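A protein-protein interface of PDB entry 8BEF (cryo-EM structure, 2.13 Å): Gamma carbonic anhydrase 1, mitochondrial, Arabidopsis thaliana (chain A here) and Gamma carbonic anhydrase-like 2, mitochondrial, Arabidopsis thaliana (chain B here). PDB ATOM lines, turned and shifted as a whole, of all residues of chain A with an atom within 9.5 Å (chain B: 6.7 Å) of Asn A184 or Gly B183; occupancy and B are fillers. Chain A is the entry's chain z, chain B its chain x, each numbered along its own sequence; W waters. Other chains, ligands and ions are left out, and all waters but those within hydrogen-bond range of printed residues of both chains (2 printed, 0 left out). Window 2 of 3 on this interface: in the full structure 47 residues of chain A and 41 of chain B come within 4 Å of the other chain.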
ATOM      1  N   VAL A 133     -25.819  12.856   5.634  1.00  0.00           N
ATOM      2  CA  VAL A 133     -26.288  11.619   6.269  1.00  0.00           C
ATOM      3  C   VAL A 133     -25.179  10.960   7.091  1.00  0.00           C
ATOM      4  O   VAL A 133     -24.175  10.596   6.548  1.00  0.00           O
ATOM      5  CB  VAL A 133     -26.938  10.636   5.278  1.00  0.00           C
ATOM      6  CG1 VAL A 133     -27.398   9.378   5.987  1.00  0.00           C
ATOM      7  CG2 VAL A 133     -28.115  11.279   4.551  1.00  0.00           C
ATOM      8  N   GLY A 148     -24.507  17.355   2.090  1.00  0.00           N
ATOM      9  CA  GLY A 148     -24.906  16.318   1.163  1.00  0.00           C
ATOM     10  C   GLY A 148     -24.034  15.082   1.168  1.00  0.00           C
ATOM     11  O   GLY A 148     -24.248  14.191   0.343  1.00  0.00           O
ATOM     12  N   ALA A 149     -23.056  15.000   2.065  1.00  0.00           N
ATOM     13  CA  ALA A 149     -22.208  13.824   2.160  1.00  0.00           C
ATOM     14  C   ALA A 149     -22.896  12.722   2.962  1.00  0.00           C
ATOM     15  O   ALA A 149     -23.784  12.973   3.781  1.00  0.00           O
ATOM     16  CB  ALA A 149     -20.868  14.176   2.801  1.00  0.00           C
ATOM     17  N   THR A 150     -22.466  11.485   2.719  1.00  0.00           N
ATOM     18  CA  THR A 150     -23.017  10.316   3.391  1.00  0.00           C
ATOM     19  C   THR A 150     -21.886   9.513   4.018  1.00  0.00           C
ATOM     20  O   THR A 150     -20.929   9.142   3.331  1.00  0.00           O
ATOM     21  CB  THR A 150     -23.813   9.438   2.418  1.00  0.00           C
ATOM     22  OG1 THR A 150     -24.846  10.217   1.801  1.00  0.00           O
ATOM     23  CG2 THR A 150     -24.441   8.258   3.141  1.00  0.00           C
ATOM     24  N   LEU A 151     -21.999   9.243   5.317  1.00  0.00           N
ATOM     25  CA  LEU A 151     -21.012   8.469   6.062  1.00  0.00           C
ATOM     26  C   LEU A 151     -21.692   7.219   6.603  1.00  0.00           C
ATOM     27  O   LEU A 151     -22.622   7.320   7.408  1.00  0.00           O
ATOM     28  CB  LEU A 151     -20.424   9.287   7.216  1.00  0.00           C
ATOM     29  CG  LEU A 151     -19.831  10.682   6.987  1.00  0.00           C
ATOM     30  CD1 LEU A 151     -18.811  11.001   8.068  1.00  0.00           C
ATOM     31  CD2 LEU A 151     -19.212  10.840   5.622  1.00  0.00           C
ATOM     32  N   LEU A 152     -21.220   6.047   6.183  1.00  0.00           N
ATOM     33  CA  LEU A 152     -21.858   4.796   6.561  1.00  0.00           C
ATOM     34  C   LEU A 152     -21.284   4.281   7.883  1.00  0.00           C
ATOM     35  O   LEU A 152     -20.431   4.916   8.506  1.00  0.00           O
ATOM     36  CB  LEU A 152     -21.722   3.777   5.432  1.00  0.00           C
ATOM     37  CG  LEU A 152     -22.344   4.215   4.100  1.00  0.00           C
ATOM     38  CD1 LEU A 152     -22.408   3.067   3.110  1.00  0.00           C
ATOM     39  CD2 LEU A 152     -23.731   4.816   4.309  1.00  0.00           C
ATOM     40  N   VAL A 163     -14.557  15.780   4.914  1.00  0.00           N
ATOM     41  CA  VAL A 163     -15.318  14.991   3.954  1.00  0.00           C
ATOM     42  C   VAL A 163     -15.985  15.974   3.005  1.00  0.00           C
ATOM     43  O   VAL A 163     -16.818  16.783   3.426  1.00  0.00           O
ATOM     44  CB  VAL A 163     -16.349  14.091   4.648  1.00  0.00           C
ATOM     45  CG1 VAL A 163     -17.202  13.363   3.620  1.00  0.00           C
ATOM     46  CG2 VAL A 163     -15.648  13.108   5.565  1.00  0.00           C
ATOM     47  N   ALA A 164     -15.606  15.918   1.732  1.00  0.00           N
ATOM     48  CA  ALA A 164     -16.069  16.906   0.769  1.00  0.00           C
ATOM     49  C   ALA A 164     -17.572  16.773   0.536  1.00  0.00           C
ATOM     50  O   ALA A 164     -18.173  15.721   0.757  1.00  0.00           O
ATOM     51  CB  ALA A 164     -15.317  16.763  -0.553  1.00  0.00           C
ATOM     52  N   ALA A 165     -18.179  17.872   0.095  1.00  0.00           N
ATOM     53  CA  ALA A 165     -19.614  17.883  -0.160  1.00  0.00           C
ATOM     54  C   ALA A 165     -19.992  16.811  -1.175  1.00  0.00           C
ATOM     55  O   ALA A 165     -19.309  16.613  -2.182  1.00  0.00           O
ATOM     56  CB  ALA A 165     -20.054  19.259  -0.655  1.00  0.00           C
ATOM     57  N   GLY A 166     -21.080  16.099  -0.885  1.00  0.00           N
ATOM     58  CA  GLY A 166     -21.564  15.054  -1.762  1.00  0.00           C
ATOM     59  C   GLY A 166     -20.759  13.775  -1.766  1.00  0.00           C
ATOM     60  O   GLY A 166     -20.994  12.922  -2.624  1.00  0.00           O
ATOM     61  N   ALA A 167     -19.818  13.609  -0.840  1.00  0.00           N
ATOM     62  CA  ALA A 167     -18.998  12.407  -0.793  1.00  0.00           C
ATOM     63  C   ALA A 167     -19.782  11.232  -0.211  1.00  0.00           C
ATOM     64  O   ALA A 167     -20.755  11.401   0.527  1.00  0.00           O
ATOM     65  CB  ALA A 167     -17.733  12.646   0.027  1.00  0.00           C
ATOM     66  N   LEU A 168     -19.337  10.023  -0.556  1.00  0.00           N
ATOM     67  CA  LEU A 168     -19.954   8.773  -0.102  1.00  0.00           C
ATOM     68  C   LEU A 168     -18.852   7.941   0.551  1.00  0.00           C
ATOM     69  O   LEU A 168     -18.150   7.187  -0.127  1.00  0.00           O
ATOM     70  CB  LEU A 168     -20.617   8.029  -1.269  1.00  0.00           C
ATOM     71  CG  LEU A 168     -21.659   6.920  -1.037  1.00  0.00           C
ATOM     72  CD1 LEU A 168     -21.121   5.725  -0.244  1.00  0.00           C
ATOM     73  CD2 LEU A 168     -22.923   7.466  -0.396  1.00  0.00           C
ATOM     74  N   VAL A 169     -18.710   8.066   1.865  1.00  0.00           N
ATOM     75  CA  VAL A 169     -17.681   7.332   2.593  1.00  0.00           C
ATOM     76  C   VAL A 169     -18.223   5.946   2.922  1.00  0.00           C
ATOM     77  O   VAL A 169     -19.178   5.806   3.690  1.00  0.00           O
ATOM     78  CB  VAL A 169     -17.243   8.075   3.856  1.00  0.00           C
ATOM     79  CG1 VAL A 169     -16.095   7.348   4.506  1.00  0.00           C
ATOM     80  CG2 VAL A 169     -16.833   9.484   3.504  1.00  0.00           C
ATOM     81  N   ARG A 170     -17.603   4.920   2.348  1.00  0.00           N
ATOM     82  CA  ARG A 170     -18.103   3.564   2.482  1.00  0.00           C
ATOM     83  C   ARG A 170     -17.842   3.027   3.887  1.00  0.00           C
ATOM     84  O   ARG A 170     -17.087   3.599   4.674  1.00  0.00           O
ATOM     85  CB  ARG A 170     -17.467   2.657   1.431  1.00  0.00           C
ATOM     86  CG  ARG A 170     -18.250   2.608   0.133  1.00  0.00           C
ATOM     87  CD  ARG A 170     -17.625   1.651  -0.852  1.00  0.00           C
ATOM     88  NE  ARG A 170     -18.615   0.744  -1.417  1.00  0.00           N
ATOM     89  CZ  ARG A 170     -18.979  -0.402  -0.861  1.00  0.00           C
ATOM     90  NH1 ARG A 170     -18.462  -0.805   0.290  1.00  0.00           N
ATOM     91  NH2 ARG A 170     -19.881  -1.163  -1.471  1.00  0.00           N
ATOM     92  N   TRP A 181     -11.226  14.027   1.615  1.00  0.00           N
ATOM     93  CA  TRP A 181     -11.730  12.885   0.865  1.00  0.00           C
ATOM     94  C   TRP A 181     -13.074  13.236   0.240  1.00  0.00           C
ATOM     95  O   TRP A 181     -13.938  13.824   0.897  1.00  0.00           O
ATOM     96  CB  TRP A 181     -11.889  11.652   1.754  1.00  0.00           C
ATOM     97  CG  TRP A 181     -10.616  11.007   2.199  1.00  0.00           C
ATOM     98  CD1 TRP A 181      -9.521  11.624   2.724  1.00  0.00           C
ATOM     99  CD2 TRP A 181     -10.320   9.608   2.183  1.00  0.00           C
ATOM    100  NE1 TRP A 181      -8.555  10.699   3.026  1.00  0.00           N
ATOM    101  CE2 TRP A 181      -9.020   9.451   2.704  1.00  0.00           C
ATOM    102  CE3 TRP A 181     -11.025   8.471   1.776  1.00  0.00           C
ATOM    103  CZ2 TRP A 181      -8.411   8.205   2.826  1.00  0.00           C
ATOM    104  CZ3 TRP A 181     -10.420   7.235   1.899  1.00  0.00           C
ATOM    105  CH2 TRP A 181      -9.125   7.112   2.418  1.00  0.00           C
ATOM    106  N   GLY A 182     -13.250  12.869  -1.031  1.00  0.00           N
ATOM    107  CA  GLY A 182     -14.485  13.164  -1.730  1.00  0.00           C
ATOM    108  C   GLY A 182     -14.756  12.174  -2.843  1.00  0.00           C
ATOM    109  O   GLY A 182     -13.930  11.315  -3.159  1.00  0.00           O
ATOM    110  N   GLY A 183     -15.940  12.309  -3.437  1.00  0.00           N
ATOM    111  CA  GLY A 183     -16.374  11.440  -4.510  1.00  0.00           C
ATOM    112  C   GLY A 183     -17.170  10.241  -4.024  1.00  0.00           C
ATOM    113  O   GLY A 183     -17.351  10.006  -2.826  1.00  0.00           O
ATOM    114  N   ASN A 184     -17.668   9.474  -4.990  1.00  0.00           N
ATOM    115  CA  ASN A 184     -18.403   8.236  -4.722  1.00  0.00           C
ATOM    116  C   ASN A 184     -17.735   7.090  -5.466  1.00  0.00           C
ATOM    117  O   ASN A 184     -17.885   6.975  -6.695  1.00  0.00           O
ATOM    118  CB  ASN A 184     -19.869   8.364  -5.137  1.00  0.00           C
ATOM    119  CG  ASN A 184     -20.690   7.137  -4.775  1.00  0.00           C
ATOM    120  OD1 ASN A 184     -20.179   6.180  -4.189  1.00  0.00           O
ATOM    121  ND2 ASN A 184     -21.969   7.160  -5.123  1.00  0.00           N
ATOM    122  N   PRO A 185     -16.993   6.213  -4.777  1.00  0.00           N
ATOM    123  CA  PRO A 185     -16.713   6.207  -3.330  1.00  0.00           C
ATOM    124  C   PRO A 185     -15.739   7.308  -2.933  1.00  0.00           C
ATOM    125  O   PRO A 185     -15.038   7.853  -3.778  1.00  0.00           O
ATOM    126  CB  PRO A 185     -16.126   4.808  -3.099  1.00  0.00           C
ATOM    127  CG  PRO A 185     -15.503   4.443  -4.407  1.00  0.00           C
ATOM    128  CD  PRO A 185     -16.407   5.043  -5.451  1.00  0.00           C
ATOM    129  N   ALA A 186     -15.690   7.667  -1.653  1.00  0.00           N
ATOM    130  CA  ALA A 186     -14.796   8.727  -1.209  1.00  0.00           C
ATOM    131  C   ALA A 186     -13.348   8.258  -1.272  1.00  0.00           C
ATOM    132  O   ALA A 186     -13.023   7.149  -0.843  1.00  0.00           O
ATOM    133  CB  ALA A 186     -15.157   9.165   0.210  1.00  0.00           C
ATOM    134  N   ARG A 187     -12.477   9.110  -1.808  1.00  0.00           N
ATOM    135  CA  ARG A 187     -11.060   8.808  -1.941  1.00  0.00           C
ATOM    136  C   ARG A 187     -10.250  10.037  -1.555  1.00  0.00           C
ATOM    137  O   ARG A 187     -10.751  11.163  -1.575  1.00  0.00           O
ATOM    138  CB  ARG A 187     -10.704   8.377  -3.369  1.00  0.00           C
ATOM    139  CG  ARG A 187     -11.099   6.957  -3.712  1.00  0.00           C
ATOM    140  CD  ARG A 187     -10.422   6.474  -4.992  1.00  0.00           C
ATOM    141  NE  ARG A 187      -9.879   7.569  -5.787  1.00  0.00           N
ATOM    142  CZ  ARG A 187      -8.589   7.860  -5.882  1.00  0.00           C
ATOM    143  NH1 ARG A 187      -7.671   7.154  -5.242  1.00  0.00           N
ATOM    144  NH2 ARG A 187      -8.209   8.888  -6.637  1.00  0.00           N
ATOM    145  N   PHE A 188      -8.987   9.806  -1.203  1.00  0.00           N
ATOM    146  CA  PHE A 188      -8.077  10.902  -0.892  1.00  0.00           C
ATOM    147  C   PHE A 188      -7.983  11.868  -2.068  1.00  0.00           C
ATOM    148  O   PHE A 188      -7.722  11.461  -3.201  1.00  0.00           O
ATOM    149  CB  PHE A 188      -6.693  10.347  -0.546  1.00  0.00           C
ATOM    150  CG  PHE A 188      -5.651  11.404  -0.337  1.00  0.00           C
ATOM    151  CD1 PHE A 188      -5.554  12.064   0.873  1.00  0.00           C
ATOM    152  CD2 PHE A 188      -4.773  11.743  -1.352  1.00  0.00           C
ATOM    153  CE1 PHE A 188      -4.601  13.040   1.070  1.00  0.00           C
ATOM    154  CE2 PHE A 188      -3.819  12.720  -1.160  1.00  0.00           C
ATOM    155  CZ  PHE A 188      -3.733  13.368   0.052  1.00  0.00           C
ATOM    156  N   LEU A 189      -8.209  13.153  -1.794  1.00  0.00           N
ATOM    157  CA  LEU A 189      -8.115  14.202  -2.801  1.00  0.00           C
ATOM    158  C   LEU A 189      -6.860  15.046  -2.649  1.00  0.00           C
ATOM    159  O   LEU A 189      -6.168  15.312  -3.635  1.00  0.00           O
ATOM    160  CB  LEU A 189      -9.349  15.116  -2.746  1.00  0.00           C
ATOM    161  CG  LEU A 189     -10.734  14.478  -2.850  1.00  0.00           C
ATOM    162  CD1 LEU A 189     -11.817  15.504  -2.559  1.00  0.00           C
ATOM    163  CD2 LEU A 189     -10.939  13.859  -4.216  1.00  0.00           C
ATOM    164  N   GLY B 163     -30.536   1.337  -1.080  1.00  0.00           N
ATOM    165  CA  GLY B 163     -29.568   1.942  -0.189  1.00  0.00           C
ATOM    166  C   GLY B 163     -29.898   3.388   0.129  1.00  0.00           C
ATOM    167  O   GLY B 163     -30.643   4.061  -0.582  1.00  0.00           O
ATOM    168  N   GLN B 164     -29.324   3.867   1.232  1.00  0.00           N
ATOM    169  CA  GLN B 164     -29.537   5.242   1.664  1.00  0.00           C
ATOM    170  C   GLN B 164     -29.109   6.228   0.582  1.00  0.00           C
ATOM    171  O   GLN B 164     -28.172   5.982  -0.178  1.00  0.00           O
ATOM    172  CB  GLN B 164     -28.748   5.531   2.943  1.00  0.00           C
ATOM    173  CG  GLN B 164     -29.354   4.966   4.208  1.00  0.00           C
ATOM    174  CD  GLN B 164     -28.464   5.190   5.413  1.00  0.00           C
ATOM    175  OE1 GLN B 164     -28.500   6.249   6.032  1.00  0.00           O
ATOM    176  NE2 GLN B 164     -27.658   4.191   5.750  1.00  0.00           N
ATOM    177  N   HIS B 165     -29.796   7.367   0.491  1.00  0.00           N
ATOM    178  CA  HIS B 165     -29.404   8.521  -0.361  1.00  0.00           C
ATOM    179  C   HIS B 165     -29.398   8.122  -1.839  1.00  0.00           C
ATOM    180  O   HIS B 165     -28.581   8.592  -2.551  1.00  0.00           O
ATOM    181  CB  HIS B 165     -28.082   9.136   0.164  1.00  0.00           C
ATOM    182  CG  HIS B 165     -28.013  10.600  -0.028  1.00  0.00           C
ATOM    183  ND1 HIS B 165     -27.429  11.171  -1.136  1.00  0.00           N
ATOM    184  CD2 HIS B 165     -28.519  11.608   0.704  1.00  0.00           C
ATOM    185  CE1 HIS B 165     -27.547  12.482  -1.053  1.00  0.00           C
ATOM    186  NE2 HIS B 165     -28.211  12.765   0.065  1.00  0.00           N
ATOM    187  N   SER B 166     -30.281   7.240  -2.223  1.00  0.00           N
ATOM    188  CA  SER B 166     -30.461   6.811  -3.615  1.00  0.00           C
ATOM    189  C   SER B 166     -31.536   7.592  -4.374  1.00  0.00           C
ATOM    190  O   SER B 166     -32.507   8.091  -3.775  1.00  0.00           O
ATOM    191  CB  SER B 166     -30.700   5.280  -3.638  1.00  0.00           C
ATOM    192  OG  SER B 166     -29.516   4.571  -3.330  1.00  0.00           O
ATOM    193  N   ILE B 167     -31.480   7.524  -5.672  1.00  0.00           N
ATOM    194  CA  ILE B 167     -32.416   8.244  -6.528  1.00  0.00           C
ATOM    195  C   ILE B 167     -32.918   7.303  -7.616  1.00  0.00           C
ATOM    196  O   ILE B 167     -32.117   6.713  -8.351  1.00  0.00           O
ATOM    197  CB  ILE B 167     -31.779   9.503  -7.141  1.00  0.00           C
ATOM    198  CG1 ILE B 167     -31.317  10.447  -6.029  1.00  0.00           C
ATOM    199  CG2 ILE B 167     -32.760  10.197  -8.072  1.00  0.00           C
ATOM    200  CD1 ILE B 167     -30.594  11.675  -6.515  1.00  0.00           C
ATOM    201  N   LEU B 180     -29.650  -2.167  -4.189  1.00  0.00           N
ATOM    202  CA  LEU B 180     -28.965  -0.976  -4.665  1.00  0.00           C
ATOM    203  C   LEU B 180     -28.117  -0.418  -3.534  1.00  0.00           C
ATOM    204  O   LEU B 180     -28.604  -0.248  -2.414  1.00  0.00           O
ATOM    205  CB  LEU B 180     -29.962   0.080  -5.144  1.00  0.00           C
ATOM    206  CG  LEU B 180     -30.277   0.119  -6.638  1.00  0.00           C
ATOM    207  CD1 LEU B 180     -31.389   1.115  -6.906  1.00  0.00           C
ATOM    208  CD2 LEU B 180     -29.036   0.465  -7.450  1.00  0.00           C
ATOM    209  N   GLU B 181     -26.850  -0.144  -3.827  1.00  0.00           N
ATOM    210  CA  GLU B 181     -25.959   0.396  -2.816  1.00  0.00           C
ATOM    211  C   GLU B 181     -26.321   1.843  -2.499  1.00  0.00           C
ATOM    212  O   GLU B 181     -26.987   2.530  -3.276  1.00  0.00           O
ATOM    213  CB  GLU B 181     -24.509   0.311  -3.282  1.00  0.00           C
ATOM    214  CG  GLU B 181     -23.888  -1.052  -3.082  1.00  0.00           C
ATOM    215  CD  GLU B 181     -22.395  -1.031  -3.279  1.00  0.00           C
ATOM    216  OE1 GLU B 181     -21.903  -0.113  -3.967  1.00  0.00           O
ATOM    217  OE2 GLU B 181     -21.714  -1.931  -2.748  1.00  0.00           O
ATOM    218  N   ALA B 182     -25.874   2.300  -1.332  1.00  0.00           N
ATOM    219  CA  ALA B 182     -26.109   3.682  -0.937  1.00  0.00           C
ATOM    220  C   ALA B 182     -25.517   4.638  -1.965  1.00  0.00           C
ATOM    221  O   ALA B 182     -24.438   4.400  -2.511  1.00  0.00           O
ATOM    222  CB  ALA B 182     -25.510   3.954   0.445  1.00  0.00           C
ATOM    223  N   GLY B 183     -26.247   5.715  -2.243  1.00  0.00           N
ATOM    224  CA  GLY B 183     -25.790   6.719  -3.179  1.00  0.00           C
ATOM    225  C   GLY B 183     -25.995   6.392  -4.640  1.00  0.00           C
ATOM    226  O   GLY B 183     -25.419   7.073  -5.494  1.00  0.00           O
ATOM    227  N   SER B 184     -26.789   5.377  -4.960  1.00  0.00           N
ATOM    228  CA  SER B 184     -27.008   5.000  -6.347  1.00  0.00           C
ATOM    229  C   SER B 184     -27.969   5.965  -7.030  1.00  0.00           C
ATOM    230  O   SER B 184     -28.881   6.517  -6.408  1.00  0.00           O
ATOM    231  CB  SER B 184     -27.552   3.576  -6.438  1.00  0.00           C
ATOM    232  OG  SER B 184     -26.679   2.651  -5.820  1.00  0.00           O
ATOM    233  N   VAL B 185     -27.709   6.188  -8.295  1.00  0.00           N
ATOM    234  CA  VAL B 185     -28.572   7.006  -9.172  1.00  0.00           C
ATOM    235  C   VAL B 185     -29.068   6.168 -10.359  1.00  0.00           C
ATOM    236  O   VAL B 185     -28.270   5.821 -11.202  1.00  0.00           O
ATOM    237  CB  VAL B 185     -27.929   8.376  -9.556  1.00  0.00           C
ATOM    238  CG1 VAL B 185     -28.813   9.194 -10.470  1.00  0.00           C
ATOM    239  CG2 VAL B 185     -27.455   9.172  -8.347  1.00  0.00           C
ATOM    240  N   GLY B 199     -24.875  -0.342  -7.981  1.00  0.00           N
ATOM    241  CA  GLY B 199     -24.471   0.854  -7.260  1.00  0.00           C
ATOM    242  C   GLY B 199     -23.749   1.816  -8.178  1.00  0.00           C
ATOM    243  O   GLY B 199     -23.335   1.464  -9.287  1.00  0.00           O
ATOM    244  N   GLY B 200     -23.607   3.045  -7.697  1.00  0.00           N
ATOM    245  CA  GLY B 200     -22.876   4.084  -8.393  1.00  0.00           C
ATOM    246  C   GLY B 200     -23.788   5.171  -8.943  1.00  0.00           C
ATOM    247  O   GLY B 200     -25.015   5.072  -8.934  1.00  0.00           O
ATOM    248  N   ASN B 201     -23.157   6.247  -9.410  1.00  0.00           N
ATOM    249  CA  ASN B 201     -23.797   7.425 -10.045  1.00  0.00           C
ATOM    250  C   ASN B 201     -23.200   7.678 -11.453  1.00  0.00           C
ATOM    251  O   ASN B 201     -22.279   8.406 -11.546  1.00  0.00           O
ATOM    252  CB  ASN B 201     -23.737   8.683  -9.162  1.00  0.00           C
ATOM    253  CG  ASN B 201     -24.448   9.852  -9.829  1.00  0.00           C
ATOM    254  OD1 ASN B 201     -24.978   9.724 -10.919  1.00  0.00           O
ATOM    255  ND2 ASN B 201     -24.499  11.000  -9.187  1.00  0.00           N
HETATM  256  O   HOH W   1     -23.183   4.253  -4.596  1.00  0.00           O
HETATM  257  O   HOH W   2     -24.329   9.126  -4.722  1.00  0.00           O
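ND2 of Asn A184 sits at hydrogen-bond distance from O of Gly B183, 3.5 Å away. OE1 of Glu B181 is in salt-bridge range of NH2 of Arg A170 (3.4 Å).
The side-chain hydroxyl of Ser B166 is in hydrogen-bond range of the backbone carbonyl oxygen of Glu B181, at 3.3 Å. O of Ala A149 lies within hydrogen-bond range of N of Val A133. The side-chain hydroxyl (OG) of Ser B184 sits at hydrogen-bond distance from the backbone carbonyl oxygen (O) of Glu B181 (2.6 Å). The backbone carbonyl oxygen of Val A133 is in hydrogen-bond range of the backbone NH of Leu A151 (2.8 Å). The backbone carbonyl oxygen (O) of Gln B164 sits at hydrogen-bond distance from the backbone NH (N) of Gly B183 (2.8 Å). The backbone carbonyl oxygen of Thr A150 lies within hydrogen-bond range of the backbone NH of Val A169 (2.9 Å).
Val A133 touches Gln B164 (CG1 to OE1, 3.3 Å). His B165 touches Val A133. Gly A148 touches His B165. Thr A150 touches His B165.
Of chain B, only Gly B183 comes within 4 Å of Asn A184. Gly B183 touches one residue of chain A. No residue of chain A comes within 4 Å of Ala B182. No residue of chain A comes within 4 Å of Ser B184. No residue of chain A comes within 4 Å of Gly B200. Printed residues of chain B within 4 Å of Arg A170: Glu B181. Printed residues of chain A within 4 Å of His B165: Val A133, Gly A148 and Thr A150. Of the printed residues of chain A, Gln B164 touches Val A133. Ser B166 touches none of the printed residues of chain A. The nearest residue of chain A that does not touch Gly B183 is Leu A168 (4.1 Å). The nearest printed residue of chain B that does not touch Gly A148 is Gly B183 (8.4 Å).
Of the 14 printed residues of chain B, 4 touch a printed residue of chain A. Printed residues of chain B that touch a printed residue of chain A: Gln B164, His B165, Glu B181 and Gly B183. Hydrophobic or aromatic side chains of chain B within 4 Å of the printed part of chain A: His B165. Of the 23 printed residues of chain A, 5 touch a printed residue of chain B. Printed residues of chain A that touch a printed residue of chain B: Val A133, Gly A148, Thr A150, Arg A170 and Asn A184. Hydrophobic or aromatic side chains of chain A that line the printed part of chain B: Val A133. Among the printed residues, Asp or Glu carboxylates within 4 Å of a Lys or Arg side-chain nitrogen of the other chain: Arg A170 with Glu B181 (2.4 Å).
Water W1 lies within hydrogen-bond range of O of Ala B182 (2.4 Å), ND2 of Asn A184 (3.2 Å) and N of Gly B200 (3.4 Å). Water W2 bridges O of Gly B183 and ND2 of Asn A184.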
